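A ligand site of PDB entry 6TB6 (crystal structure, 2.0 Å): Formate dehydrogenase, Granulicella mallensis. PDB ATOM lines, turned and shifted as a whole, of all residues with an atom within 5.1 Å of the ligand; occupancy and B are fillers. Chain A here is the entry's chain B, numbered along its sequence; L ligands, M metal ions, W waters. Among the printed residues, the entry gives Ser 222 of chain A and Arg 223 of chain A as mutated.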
ATOM      1  N   PHE A  99      12.974 -18.545  39.696  1.00  0.00           N
ATOM      2  CA  PHE A  99      13.740 -19.432  40.568  1.00  0.00           C
ATOM      3  C   PHE A  99      12.905 -20.599  41.053  1.00  0.00           C
ATOM      4  O   PHE A  99      13.454 -21.639  41.415  1.00  0.00           O
ATOM      5  CB  PHE A  99      14.292 -18.619  41.755  1.00  0.00           C
ATOM      6  CG  PHE A  99      14.602 -17.225  41.364  1.00  0.00           C
ATOM      7  CD1 PHE A  99      15.647 -16.977  40.501  1.00  0.00           C
ATOM      8  CD2 PHE A  99      13.771 -16.192  41.728  1.00  0.00           C
ATOM      9  CE1 PHE A  99      15.883 -15.713  40.062  1.00  0.00           C
ATOM     10  CE2 PHE A  99      13.991 -14.931  41.278  1.00  0.00           C
ATOM     11  CZ  PHE A  99      15.052 -14.682  40.442  1.00  0.00           C
ATOM     12  N   ILE A 123      13.195 -11.735  35.862  1.00  0.00           N
ATOM     13  CA  ILE A 123      13.429 -11.406  34.446  1.00  0.00           C
ATOM     14  C   ILE A 123      13.448 -12.700  33.643  1.00  0.00           C
ATOM     15  O   ILE A 123      14.099 -13.672  34.032  1.00  0.00           O
ATOM     16  CB  ILE A 123      14.757 -10.643  34.272  1.00  0.00           C
ATOM     17  CG1 ILE A 123      14.694  -9.257  34.915  1.00  0.00           C
ATOM     18  CG2 ILE A 123      15.102 -10.496  32.808  1.00  0.00           C
ATOM     19  CD1 ILE A 123      16.029  -8.534  34.921  1.00  0.00           C
ATOM     20  N   GLY A 124      12.743 -12.722  32.511  1.00  0.00           N
ATOM     21  CA  GLY A 124      12.681 -13.892  31.659  1.00  0.00           C
ATOM     22  C   GLY A 124      11.379 -14.643  31.862  1.00  0.00           C
ATOM     23  O   GLY A 124      11.181 -15.287  32.901  1.00  0.00           O
ATOM     24  N   ASP A 126       9.992 -17.083  29.816  1.00  0.00           N
ATOM     25  CA  ASP A 126       9.915 -18.333  29.064  1.00  0.00           C
ATOM     26  C   ASP A 126       9.056 -19.396  29.709  1.00  0.00           C
ATOM     27  O   ASP A 126       8.729 -20.380  29.036  1.00  0.00           O
ATOM     28  CB  ASP A 126      11.324 -18.908  28.864  1.00  0.00           C
ATOM     29  CG  ASP A 126      12.132 -18.894  30.134  1.00  0.00           C
ATOM     30  OD1 ASP A 126      12.713 -17.832  30.437  1.00  0.00           O
ATOM     31  OD2 ASP A 126      12.156 -19.935  30.805  1.00  0.00           O
ATOM     32  N   ASN A 147      17.402  -7.499  38.269  1.00  0.00           N
ATOM     33  CA  ASN A 147      18.489  -8.313  38.802  1.00  0.00           C
ATOM     34  C   ASN A 147      19.576  -8.564  37.752  1.00  0.00           C
ATOM     35  O   ASN A 147      20.422  -9.456  37.926  1.00  0.00           O
ATOM     36  CB  ASN A 147      17.954  -9.632  39.349  1.00  0.00           C
ATOM     37  CG  ASN A 147      17.159 -10.448  38.297  1.00  0.00           C
ATOM     38  OD1 ASN A 147      17.252 -10.192  37.107  1.00  0.00           O
ATOM     39  ND2 ASN A 147      16.405 -11.420  38.763  1.00  0.00           N
ATOM     40  N   SER A 148      19.600  -7.771  36.685  1.00  0.00           N
ATOM     41  CA  SER A 148      20.592  -7.957  35.643  1.00  0.00           C
ATOM     42  C   SER A 148      22.015  -7.797  36.183  1.00  0.00           C
ATOM     43  O   SER A 148      22.918  -8.540  35.801  1.00  0.00           O
ATOM     44  CB  SER A 148      20.320  -6.986  34.499  1.00  0.00           C
ATOM     45  OG  SER A 148      19.005  -7.160  33.987  1.00  0.00           O
ATOM     46  N   VAL A 151      23.218 -10.869  38.280  1.00  0.00           N
ATOM     47  CA  VAL A 151      23.693 -11.983  37.476  1.00  0.00           C
ATOM     48  C   VAL A 151      25.103 -11.714  36.969  1.00  0.00           C
ATOM     49  O   VAL A 151      25.950 -12.611  36.984  1.00  0.00           O
ATOM     50  CB  VAL A 151      22.737 -12.263  36.306  1.00  0.00           C
ATOM     51  CG1 VAL A 151      23.218 -13.446  35.481  1.00  0.00           C
ATOM     52  CG2 VAL A 151      21.344 -12.504  36.869  1.00  0.00           C
ATOM     53  N   VAL A 198      27.603 -14.499  24.661  1.00  0.00           N
ATOM     54  CA  VAL A 198      26.460 -14.670  23.761  1.00  0.00           C
ATOM     55  C   VAL A 198      25.408 -13.694  24.316  1.00  0.00           C
ATOM     56  O   VAL A 198      24.961 -13.974  25.400  1.00  0.00           O
ATOM     57  CB  VAL A 198      25.960 -16.115  23.730  1.00  0.00           C
ATOM     58  CG1 VAL A 198      24.705 -16.221  22.897  1.00  0.00           C
ATOM     59  CG2 VAL A 198      27.044 -17.059  23.224  1.00  0.00           C
ATOM     60  N   ALA A 199      25.160 -12.572  23.622  1.00  0.00           N
ATOM     61  CA  ALA A 199      24.249 -11.430  23.888  1.00  0.00           C
ATOM     62  C   ALA A 199      25.007 -10.330  24.670  1.00  0.00           C
ATOM     63  O   ALA A 199      25.836 -10.641  25.499  1.00  0.00           O
ATOM     64  CB  ALA A 199      22.914 -11.743  24.548  1.00  0.00           C
ATOM     65  N   ALA A 200      24.744  -9.074  24.344  1.00  0.00           N
ATOM     66  CA  ALA A 200      25.314  -7.887  24.996  1.00  0.00           C
ATOM     67  C   ALA A 200      24.136  -7.016  25.427  1.00  0.00           C
ATOM     68  O   ALA A 200      24.153  -5.860  25.231  1.00  0.00           O
ATOM     69  CB  ALA A 200      26.283  -7.177  24.094  1.00  0.00           C
ATOM     70  N   GLY A 201      23.174  -7.610  26.124  1.00  0.00           N
ATOM     71  CA  GLY A 201      22.022  -6.926  26.703  1.00  0.00           C
ATOM     72  C   GLY A 201      22.332  -6.376  28.072  1.00  0.00           C
ATOM     73  O   GLY A 201      23.460  -6.073  28.366  1.00  0.00           O
ATOM     74  N   ARG A 202      21.347  -6.258  28.929  1.00  0.00           N
ATOM     75  CA  ARG A 202      21.598  -5.649  30.221  1.00  0.00           C
ATOM     76  C   ARG A 202      22.610  -6.476  31.024  1.00  0.00           C
ATOM     77  O   ARG A 202      23.526  -5.913  31.627  1.00  0.00           O
ATOM     78  CB  ARG A 202      20.269  -5.468  30.965  1.00  0.00           C
ATOM     79  CG  ARG A 202      19.438  -4.310  30.400  1.00  0.00           C
ATOM     80  CD  ARG A 202      17.956  -4.392  30.808  1.00  0.00           C
ATOM     81  NE  ARG A 202      17.125  -3.377  30.148  1.00  0.00           N
ATOM     82  CZ  ARG A 202      16.320  -3.614  29.122  1.00  0.00           C
ATOM     83  NH1 ARG A 202      16.225  -4.829  28.598  1.00  0.00           N
ATOM     84  NH2 ARG A 202      15.602  -2.627  28.593  1.00  0.00           N
ATOM     85  N   ILE A 203      22.483  -7.811  31.028  1.00  0.00           N
ATOM     86  CA  ILE A 203      23.461  -8.656  31.726  1.00  0.00           C
ATOM     87  C   ILE A 203      24.774  -8.724  30.951  1.00  0.00           C
ATOM     88  O   ILE A 203      25.861  -8.549  31.505  1.00  0.00           O
ATOM     89  CB  ILE A 203      22.897 -10.066  31.971  1.00  0.00           C
ATOM     90  CG1 ILE A 203      21.684  -9.985  32.881  1.00  0.00           C
ATOM     91  CG2 ILE A 203      24.004 -10.969  32.537  1.00  0.00           C
ATOM     92  CD1 ILE A 203      20.925 -11.327  33.047  1.00  0.00           C
ATOM     93  N   GLY A 204      24.686  -8.982  29.633  1.00  0.00           N
ATOM     94  CA  GLY A 204      25.893  -9.183  28.858  1.00  0.00           C
ATOM     95  C   GLY A 204      26.823  -7.979  28.828  1.00  0.00           C
ATOM     96  O   GLY A 204      28.038  -8.126  28.912  1.00  0.00           O
ATOM     97  N   PHE A 221      28.885 -11.880  20.520  1.00  0.00           N
ATOM     98  CA  PHE A 221      27.953 -12.150  19.438  1.00  0.00           C
ATOM     99  C   PHE A 221      26.603 -11.577  19.821  1.00  0.00           C
ATOM    100  O   PHE A 221      26.123 -11.821  20.940  1.00  0.00           O
ATOM    101  CB  PHE A 221      27.843 -13.639  19.146  1.00  0.00           C
ATOM    102  CG  PHE A 221      26.614 -13.990  18.355  1.00  0.00           C
ATOM    103  CD1 PHE A 221      26.476 -13.573  17.035  1.00  0.00           C
ATOM    104  CD2 PHE A 221      25.569 -14.700  18.941  1.00  0.00           C
ATOM    105  CE1 PHE A 221      25.325 -13.885  16.298  1.00  0.00           C
ATOM    106  CE2 PHE A 221      24.426 -15.010  18.209  1.00  0.00           C
ATOM    107  CZ  PHE A 221      24.315 -14.599  16.888  1.00  0.00           C
ATOM    108  N   SER A 222      26.020 -10.804  18.917  1.00  0.00           N
ATOM    109  CA  SER A 222      24.725 -10.158  19.091  1.00  0.00           C
ATOM    110  C   SER A 222      24.077 -10.058  17.716  1.00  0.00           C
ATOM    111  O   SER A 222      24.759  -9.996  16.702  1.00  0.00           O
ATOM    112  CB  SER A 222      24.877  -8.773  19.711  1.00  0.00           C
ATOM    113  OG  SER A 222      23.613  -8.192  19.985  1.00  0.00           O
ATOM    114  N   ARG A 223      22.748  -9.955  17.685  1.00  0.00           N
ATOM    115  CA  ARG A 223      22.010  -9.736  16.419  1.00  0.00           C
ATOM    116  C   ARG A 223      22.355  -8.321  15.970  1.00  0.00           C
ATOM    117  O   ARG A 223      22.658  -8.154  14.827  1.00  0.00           O
ATOM    118  CB  ARG A 223      20.510  -9.993  16.606  1.00  0.00           C
ATOM    119  CG  ARG A 223      20.170 -11.440  16.933  1.00  0.00           C
ATOM    120  CD  ARG A 223      19.447 -12.163  15.820  1.00  0.00           C
ATOM    121  NE  ARG A 223      18.120 -12.558  16.247  1.00  0.00           N
ATOM    122  CZ  ARG A 223      17.068 -12.757  15.473  1.00  0.00           C
ATOM    123  NH1 ARG A 223      15.933 -13.117  16.041  1.00  0.00           N
ATOM    124  NH2 ARG A 223      17.124 -12.602  14.172  1.00  0.00           N
ATOM    125  N   HIS A 224      22.379  -7.362  16.890  1.00  0.00           N
ATOM    126  CA  HIS A 224      22.724  -5.979  16.595  1.00  0.00           C
ATOM    127  C   HIS A 224      23.988  -5.578  17.338  1.00  0.00           C
ATOM    128  O   HIS A 224      24.167  -5.942  18.493  1.00  0.00           O
ATOM    129  CB  HIS A 224      21.572  -5.030  16.965  1.00  0.00           C
ATOM    130  CG  HIS A 224      20.268  -5.385  16.335  1.00  0.00           C
ATOM    131  ND1 HIS A 224      20.060  -5.264  14.980  1.00  0.00           N
ATOM    132  CD2 HIS A 224      19.137  -5.916  16.845  1.00  0.00           C
ATOM    133  CE1 HIS A 224      18.844  -5.679  14.687  1.00  0.00           C
ATOM    134  NE2 HIS A 224      18.260  -6.078  15.809  1.00  0.00           N
ATOM    135  N   ASN A 255      24.316 -15.174  27.859  1.00  0.00           N
ATOM    136  CA  ASN A 255      23.489 -14.160  28.505  1.00  0.00           C
ATOM    137  C   ASN A 255      22.282 -13.772  27.643  1.00  0.00           C
ATOM    138  O   ASN A 255      21.788 -12.637  27.721  1.00  0.00           O
ATOM    139  CB  ASN A 255      24.351 -12.942  28.837  1.00  0.00           C
ATOM    140  CG  ASN A 255      25.500 -13.295  29.789  1.00  0.00           C
ATOM    141  OD1 ASN A 255      26.679 -13.295  29.416  1.00  0.00           O
ATOM    142  ND2 ASN A 255      25.125 -13.632  31.001  1.00  0.00           N
ATOM    143  N   ALA A 256      21.791 -14.692  26.846  1.00  0.00           N
ATOM    144  CA  ALA A 256      20.650 -14.440  25.985  1.00  0.00           C
ATOM    145  C   ALA A 256      19.387 -15.077  26.558  1.00  0.00           C
ATOM    146  O   ALA A 256      19.472 -16.056  27.298  1.00  0.00           O
ATOM    147  CB  ALA A 256      20.908 -14.993  24.585  1.00  0.00           C
ATOM    148  N   PRO A 257      18.199 -14.560  26.230  1.00  0.00           N
ATOM    149  CA  PRO A 257      16.967 -15.205  26.672  1.00  0.00           C
ATOM    150  C   PRO A 257      16.754 -16.536  25.964  1.00  0.00           C
ATOM    151  O   PRO A 257      17.338 -16.801  24.911  1.00  0.00           O
ATOM    152  CB  PRO A 257      15.850 -14.215  26.305  1.00  0.00           C
ATOM    153  CG  PRO A 257      16.500 -13.080  25.581  1.00  0.00           C
ATOM    154  CD  PRO A 257      17.946 -13.419  25.341  1.00  0.00           C
ATOM    155  N   LEU A 258      15.884 -17.348  26.562  1.00  0.00           N
ATOM    156  CA  LEU A 258      15.471 -18.603  25.956  1.00  0.00           C
ATOM    157  C   LEU A 258      14.370 -18.306  24.935  1.00  0.00           C
ATOM    158  O   LEU A 258      13.296 -17.817  25.286  1.00  0.00           O
ATOM    159  CB  LEU A 258      14.974 -19.580  27.013  1.00  0.00           C
ATOM    160  CG  LEU A 258      14.506 -20.950  26.558  1.00  0.00           C
ATOM    161  CD1 LEU A 258      15.614 -21.673  25.789  1.00  0.00           C
ATOM    162  CD2 LEU A 258      14.066 -21.743  27.760  1.00  0.00           C
ATOM    163  N   HIS A 259      14.625 -18.650  23.686  1.00  0.00           N
ATOM    164  CA  HIS A 259      13.624 -18.565  22.643  1.00  0.00           C
ATOM    165  C   HIS A 259      14.040 -19.524  21.536  1.00  0.00           C
ATOM    166  O   HIS A 259      15.101 -20.143  21.617  1.00  0.00           O
ATOM    167  CB  HIS A 259      13.470 -17.126  22.137  1.00  0.00           C
ATOM    168  CG  HIS A 259      14.703 -16.571  21.491  1.00  0.00           C
ATOM    169  ND1 HIS A 259      15.171 -17.022  20.274  1.00  0.00           N
ATOM    170  CD2 HIS A 259      15.549 -15.601  21.890  1.00  0.00           C
ATOM    171  CE1 HIS A 259      16.265 -16.359  19.953  1.00  0.00           C
ATOM    172  NE2 HIS A 259      16.522 -15.481  20.920  1.00  0.00           N
ATOM    173  N   GLY A 261      15.487 -19.526  18.774  1.00  0.00           N
ATOM    174  CA  GLY A 261      16.847 -19.375  18.289  1.00  0.00           C
ATOM    175  C   GLY A 261      17.942 -19.759  19.275  1.00  0.00           C
ATOM    176  O   GLY A 261      19.062 -19.988  18.845  1.00  0.00           O
ATOM    177  N   THR A 262      17.647 -19.813  20.584  1.00  0.00           N
ATOM    178  CA  THR A 262      18.677 -20.222  21.547  1.00  0.00           C
ATOM    179  C   THR A 262      18.392 -21.565  22.206  1.00  0.00           C
ATOM    180  O   THR A 262      19.257 -22.081  22.924  1.00  0.00           O
ATOM    181  CB  THR A 262      18.847 -19.152  22.649  1.00  0.00           C
ATOM    182  OG1 THR A 262      17.595 -18.959  23.332  1.00  0.00           O
ATOM    183  CG2 THR A 262      19.285 -17.827  22.044  1.00  0.00           C
ATOM    184  N   THR A 283      24.244 -18.533  33.061  1.00  0.00           N
ATOM    185  CA  THR A 283      23.242 -18.047  34.037  1.00  0.00           C
ATOM    186  C   THR A 283      22.114 -17.375  33.255  1.00  0.00           C
ATOM    187  O   THR A 283      21.569 -16.373  33.751  1.00  0.00           O
ATOM    188  CB  THR A 283      23.887 -17.104  35.067  1.00  0.00           C
ATOM    189  OG1 THR A 283      24.245 -15.901  34.403  1.00  0.00           O
ATOM    190  CG2 THR A 283      25.100 -17.710  35.743  1.00  0.00           C
ATOM    191  N   ALA A 284      21.792 -17.908  32.058  1.00  0.00           N
ATOM    192  CA  ALA A 284      20.761 -17.380  31.146  1.00  0.00           C
ATOM    193  C   ALA A 284      19.482 -18.230  31.259  1.00  0.00           C
ATOM    194  O   ALA A 284      18.491 -17.737  31.811  1.00  0.00           O
ATOM    195  CB  ALA A 284      21.304 -17.310  29.726  1.00  0.00           C
ATOM    196  N   ARG A 285      19.514 -19.488  30.798  1.00  0.00           N
ATOM    197  CA  ARG A 285      18.360 -20.434  30.816  1.00  0.00           C
ATOM    198  C   ARG A 285      18.961 -21.808  30.519  1.00  0.00           C
ATOM    199  O   ARG A 285      19.546 -21.947  29.425  1.00  0.00           O
ATOM    200  CB  ARG A 285      17.297 -20.019  29.792  1.00  0.00           C
ATOM    201  CG  ARG A 285      16.071 -19.358  30.413  1.00  0.00           C
ATOM    202  CD  ARG A 285      15.552 -20.118  31.629  1.00  0.00           C
ATOM    203  NE  ARG A 285      14.556 -19.369  32.372  1.00  0.00           N
ATOM    204  CZ  ARG A 285      14.797 -18.229  33.013  1.00  0.00           C
ATOM    205  NH1 ARG A 285      16.011 -17.701  33.006  1.00  0.00           N
ATOM    206  NH2 ARG A 285      13.830 -17.624  33.671  1.00  0.00           N
ATOM    207  N   ASP A 309      23.754 -21.155  37.258  1.00  0.00           N
ATOM    208  CA  ASP A 309      22.731 -21.293  38.287  1.00  0.00           C
ATOM    209  C   ASP A 309      21.394 -21.768  37.724  1.00  0.00           C
ATOM    210  O   ASP A 309      20.485 -22.063  38.499  1.00  0.00           O
ATOM    211  CB  ASP A 309      22.543 -19.968  39.057  1.00  0.00           C
ATOM    212  CG  ASP A 309      22.091 -18.771  38.168  1.00  0.00           C
ATOM    213  OD1 ASP A 309      22.362 -18.731  36.951  1.00  0.00           O
ATOM    214  OD2 ASP A 309      21.485 -17.826  38.753  1.00  0.00           O
ATOM    215  N   VAL A 310      21.285 -21.920  36.404  1.00  0.00           N
ATOM    216  CA  VAL A 310      20.011 -22.224  35.750  1.00  0.00           C
ATOM    217  C   VAL A 310      20.026 -23.640  35.204  1.00  0.00           C
ATOM    218  O   VAL A 310      21.023 -24.088  34.612  1.00  0.00           O
ATOM    219  CB  VAL A 310      19.680 -21.202  34.638  1.00  0.00           C
ATOM    220  CG1 VAL A 310      19.395 -19.863  35.258  1.00  0.00           C
ATOM    221  CG2 VAL A 310      20.804 -21.097  33.599  1.00  0.00           C
ATOM    222  N   HIS A 333      19.308 -22.034  41.220  1.00  0.00           N
ATOM    223  CA  HIS A 333      18.981 -20.776  40.543  1.00  0.00           C
ATOM    224  C   HIS A 333      18.820 -19.669  41.574  1.00  0.00           C
ATOM    225  O   HIS A 333      17.719 -19.417  42.093  1.00  0.00           O
ATOM    226  CB  HIS A 333      17.742 -20.969  39.680  1.00  0.00           C
ATOM    227  CG  HIS A 333      17.394 -19.784  38.842  1.00  0.00           C
ATOM    228  ND1 HIS A 333      16.209 -19.705  38.135  1.00  0.00           N
ATOM    229  CD2 HIS A 333      18.059 -18.627  38.604  1.00  0.00           C
ATOM    230  CE1 HIS A 333      16.173 -18.550  37.480  1.00  0.00           C
ATOM    231  NE2 HIS A 333      17.279 -17.881  37.743  1.00  0.00           N
ATOM    232  N   ILE A 334      19.930 -18.997  41.883  1.00  0.00           N
ATOM    233  CA  ILE A 334      19.964 -18.024  42.979  1.00  0.00           C
ATOM    234  C   ILE A 334      20.455 -16.658  42.569  1.00  0.00           C
ATOM    235  O   ILE A 334      20.228 -15.687  43.312  1.00  0.00           O
ATOM    236  CB  ILE A 334      20.807 -18.550  44.159  1.00  0.00           C
ATOM    237  CG1 ILE A 334      22.268 -18.781  43.739  1.00  0.00           C
ATOM    238  CG2 ILE A 334      20.172 -19.827  44.711  1.00  0.00           C
ATOM    239  CD1 ILE A 334      23.258 -18.800  44.920  1.00  0.00           C
ATOM    240  N   SER A 335      21.142 -16.456  41.433  1.00  0.00           N
ATOM    241  CA  SER A 335      21.820 -15.183  41.245  1.00  0.00           C
ATOM    242  C   SER A 335      20.821 -14.031  41.208  1.00  0.00           C
ATOM    243  O   SER A 335      21.055 -12.976  41.797  1.00  0.00           O
ATOM    244  CB  SER A 335      22.678 -15.189  39.967  1.00  0.00           C
ATOM    245  OG  SER A 335      21.936 -15.181  38.754  1.00  0.00           O
ATOM    246  N   GLY A 336      19.713 -14.212  40.492  1.00  0.00           N
ATOM    247  CA  GLY A 336      18.695 -13.201  40.402  1.00  0.00           C
ATOM    248  C   GLY A 336      17.820 -13.041  41.619  1.00  0.00           C
ATOM    249  O   GLY A 336      16.935 -12.183  41.584  1.00  0.00           O
ATOM    250  N   THR A 337      18.053 -13.789  42.697  1.00  0.00           N
ATOM    251  CA  THR A 337      17.254 -13.650  43.920  1.00  0.00           C
ATOM    252  C   THR A 337      18.168 -13.528  45.146  1.00  0.00           C
ATOM    253  O   THR A 337      17.863 -14.005  46.248  1.00  0.00           O
ATOM    254  CB  THR A 337      16.240 -14.797  44.032  1.00  0.00           C
ATOM    255  OG1 THR A 337      15.230 -14.466  45.017  1.00  0.00           O
ATOM    256  CG2 THR A 337      16.878 -16.133  44.361  1.00  0.00           C
HETATM  257  P1  LIG L   1      17.954  -8.109  27.985  1.00  0.00           P
HETATM  258  O1  LIG L   1      16.609  -8.182  27.290  1.00  0.00           O
HETATM  259  O2  LIG L   1      18.396  -6.724  28.437  1.00  0.00           O
HETATM  260  O3  LIG L   1      19.158  -8.635  27.015  1.00  0.00           O
HETATM  261  C1  LIG L   1      18.896  -9.767  26.278  1.00  0.00           C
HETATM  262  C2  LIG L   1      19.753  -9.562  24.987  1.00  0.00           C
HETATM  263  O4  LIG L   1      19.804 -10.964  24.331  1.00  0.00           O
HETATM  264  C3  LIG L   1      19.216  -8.769  24.154  1.00  0.00           C
HETATM  265  O5  LIG L   1      20.170  -7.667  23.858  1.00  0.00           O
HETATM  266  C4  LIG L   1      18.948  -9.641  22.774  1.00  0.00           C
HETATM  267  O6  LIG L   1      19.115  -8.723  21.640  1.00  0.00           O
HETATM  268  C5  LIG L   1      19.887 -10.515  22.881  1.00  0.00           C
HETATM  269  N1  LIG L   1      19.999 -11.806  22.067  1.00  0.00           N
HETATM  270  C6  LIG L   1      18.748 -12.268  21.910  1.00  0.00           C
HETATM  271  N2  LIG L   1      18.830 -13.436  21.207  1.00  0.00           N
HETATM  272  C7  LIG L   1      20.136 -13.676  20.959  1.00  0.00           C
HETATM  273  C8  LIG L   1      20.843 -14.668  20.298  1.00  0.00           C
HETATM  274  N3  LIG L   1      20.111 -15.777  19.677  1.00  0.00           N
HETATM  275  N4  LIG L   1      22.163 -14.592  20.231  1.00  0.00           N
HETATM  276  C9  LIG L   1      22.857 -13.549  20.805  1.00  0.00           C
HETATM  277  N5  LIG L   1      22.186 -12.579  21.437  1.00  0.00           N
HETATM  278  C10 LIG L   1      20.843 -12.662  21.505  1.00  0.00           C
HETATM  279  O7  LIG L   1      17.716  -9.147  29.259  1.00  0.00           O
HETATM  280  P2  LIG L   1      18.816  -9.446  30.443  1.00  0.00           P
HETATM  281  O8  LIG L   1      20.219  -9.218  29.943  1.00  0.00           O
HETATM  282  O9  LIG L   1      18.475  -8.558  31.589  1.00  0.00           O
HETATM  283  O10 LIG L   1      18.582 -11.031  30.822  1.00  0.00           O
HETATM  284  C11 LIG L   1      18.796 -11.924  29.735  1.00  0.00           C
HETATM  285  C12 LIG L   1      18.164 -13.231  30.044  1.00  0.00           C
HETATM  286  O11 LIG L   1      18.977 -13.818  31.269  1.00  0.00           O
HETATM  287  C13 LIG L   1      16.902 -13.196  30.455  1.00  0.00           C
HETATM  288  O12 LIG L   1      15.966 -13.392  29.319  1.00  0.00           O
HETATM  289  C14 LIG L   1      16.757 -14.383  31.378  1.00  0.00           C
HETATM  290  O13 LIG L   1      16.429 -15.559  30.731  1.00  0.00           O
HETATM  291  C15 LIG L   1      18.196 -14.556  31.965  1.00  0.00           C
HETATM  292  N6  LIG L   1      18.225 -14.132  33.402  1.00  0.00           N
HETATM  293  C16 LIG L   1      18.697 -14.987  34.313  1.00  0.00           C
HETATM  294  C17 LIG L   1      18.723 -14.619  35.667  1.00  0.00           C
HETATM  295  C18 LIG L   1      19.286 -15.577  36.710  1.00  0.00           C
HETATM  296  O14 LIG L   1      20.171 -16.390  36.449  1.00  0.00           O
HETATM  297  N7  LIG L   1      18.790 -15.441  38.015  1.00  0.00           N
HETATM  298  C19 LIG L   1      18.279 -13.392  36.036  1.00  0.00           C
HETATM  299  C20 LIG L   1      17.809 -12.518  35.099  1.00  0.00           C
HETATM  300  C21 LIG L   1      17.778 -12.883  33.768  1.00  0.00           C
HETATM  301  P3  LIG L   1      17.820  -8.359  20.644  1.00  0.00           P
HETATM  302  O15 LIG L   1      18.400  -8.167  19.291  1.00  0.00           O
HETATM  303  O16 LIG L   1      16.827  -9.522  20.607  1.00  0.00           O
HETATM  304  O17 LIG L   1      17.150  -7.085  21.055  1.00  0.00           O
HETATM  305 CO    CO M   1      16.394  -6.898  16.186  1.00  0.00          CO
HETATM  306 CO    CO M   2      13.673 -11.312  22.266  1.00  0.00          CO
HETATM  307  O   HOH W   1      13.879 -11.356  29.173  1.00  0.00           O
HETATM  308  O   HOH W   2      14.320 -16.260  28.897  1.00  0.00           O
HETATM  309  O   HOH W   3      14.223  -9.274  21.522  1.00  0.00           O
HETATM  310  O   HOH W   4      18.931  -5.101  26.321  1.00  0.00           O
HETATM  311  O   HOH W   5      22.322  -9.848  28.181  1.00  0.00           O
HETATM  312  O   HOH W   6      15.917  -7.075  31.937  1.00  0.00           O
HETATM  313  O   HOH W   7      22.605  -8.393  22.504  1.00  0.00           O
HETATM  314  O   HOH W   8      20.872  -7.887  19.428  1.00  0.00           O
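The backbone NH of Ile 203 lies within hydrogen-bond range of an oxygen (O8) of the ligand (2.9 Å).
N of Arg 202 sits at hydrogen-bond distance from O2 of the ligand (3.0 Å).
OG of Ser 148 sits at hydrogen-bond distance from O9 of the ligand (2.8 Å).
The side-chain hydroxyl (OG) of Ser 335 lies within hydrogen-bond range of an oxygen (O14) of the ligand.
An oxygen (O13) of the ligand sits at hydrogen-bond distance from the backbone carbonyl oxygen of Ala 284 (3.2 Å).
A nitrogen (N2) of the ligand is in hydrogen-bond range of a ring nitrogen (NE2) of His 259, at 3.1 Å.
A nitrogen (N7) of the ligand sits at hydrogen-bond distance from a ring nitrogen (NE2) of His 333, 2.9 Å away.
An oxygen (O13) of the ligand is in hydrogen-bond range of the guanidinium group (NH1) of Arg 285 (3.2 Å).
An oxygen (O2) of the ligand is in salt-bridge range of the guanidinium group of Arg 202 (2.9 Å).
The backbone carbonyl oxygen (O) of Gly 336 sits at hydrogen-bond distance from the side-chain amide nitrogen (ND2) of Asn 147 (3.0 Å).
The side-chain hydroxyl (OG) of Ser 222 lies within hydrogen-bond range of the backbone carbonyl oxygen (O) of His 224.
The side-chain carboxylate of Asp 309 sits at hydrogen-bond distance from the side-chain hydroxyl of Ser 335, 2.7 Å away.
N of Ala 199 is in hydrogen-bond range of O of Phe 221 (2.9 Å).
NE of Arg 285 lies within salt-bridge range of OD2 of Asp 126, 2.9 Å away.
N of His 333 sits close to O of Asp 309 (3.0 Å).
N of His 259 lies within hydrogen-bond range of OG1 of Thr 262, at 3.0 Å.
The backbone NH (N) of Asn 255 sits at hydrogen-bond distance from the backbone carbonyl oxygen (O) of Val 198.
An oxygen (O14) of the ligand sits close to the backbone carbonyl oxygen (O) of Thr 283, at 3.0 Å.
The side-chain carboxylate (OD2) of Asp 309 sits close to an oxygen (O14) of the ligand (3.0 Å).
N7 of the ligand lies close to N of Gly 336 (2.9 Å).
Merely in contact with the ligand: Phe 221 (3.1 Å), Asn 147 (3.1 Å), Pro 257 (3.1 Å), Ala 199 (3.2 Å), Thr 262 (3.2 Å), Val 151 (3.3 Å), Gly 201 (3.3 Å), His 224 (3.4 Å), Phe 99 (3.6 Å), Ile 123 (3.7 Å), Asn 255 (3.7 Å), Val 310 (3.8 Å), Ala 256 (3.9 Å), Val 198 (3.9 Å) and Arg 223 (3.9 Å).
Hydrophobic or aromatic side chains that line the ligand: Phe 99, Ile 123, Val 151, Val 198, Ala 199, Ile 203, Phe 221, His 224, Ala 256, Pro 257, His 259, Val 310 and His 333.
Within 4 Å of the ligand: Phe 99, Ile 123, Asn 147, Ser 148, Val 151, Val 198, Ala 199, Gly 201, Arg 202, Ile 203, Phe 221, Arg 223, His 224, Asn 255, Ala 256, Pro 257, His 259, Thr 262, Thr 283, Ala 284, Arg 285, Asp 309, Val 310, His 333, Ser 335 and Gly 336.
Water W8 lies within hydrogen-bond range of an oxygen (O15) of the ligand (2.5 Å), the side-chain hydroxyl of Ser 222 (2.8 Å), the backbone NH of His 224 (3.0 Å) and the backbone NH of Arg 223 (3.3 Å).
Water W5 lies within hydrogen-bond range of O8 of the ligand (2.8 Å), O of Asn 255 (2.9 Å), N of Gly 204 (2.9 Å) and N of Gly 201 (3.2 Å).
Water W7 lies within hydrogen-bond range of OG of Ser 222, O5 of the ligand and N of Ala 200.
Water W2 lies within hydrogen-bond range of OD1 of Asp 126, O13 of the ligand and N of Leu 258.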
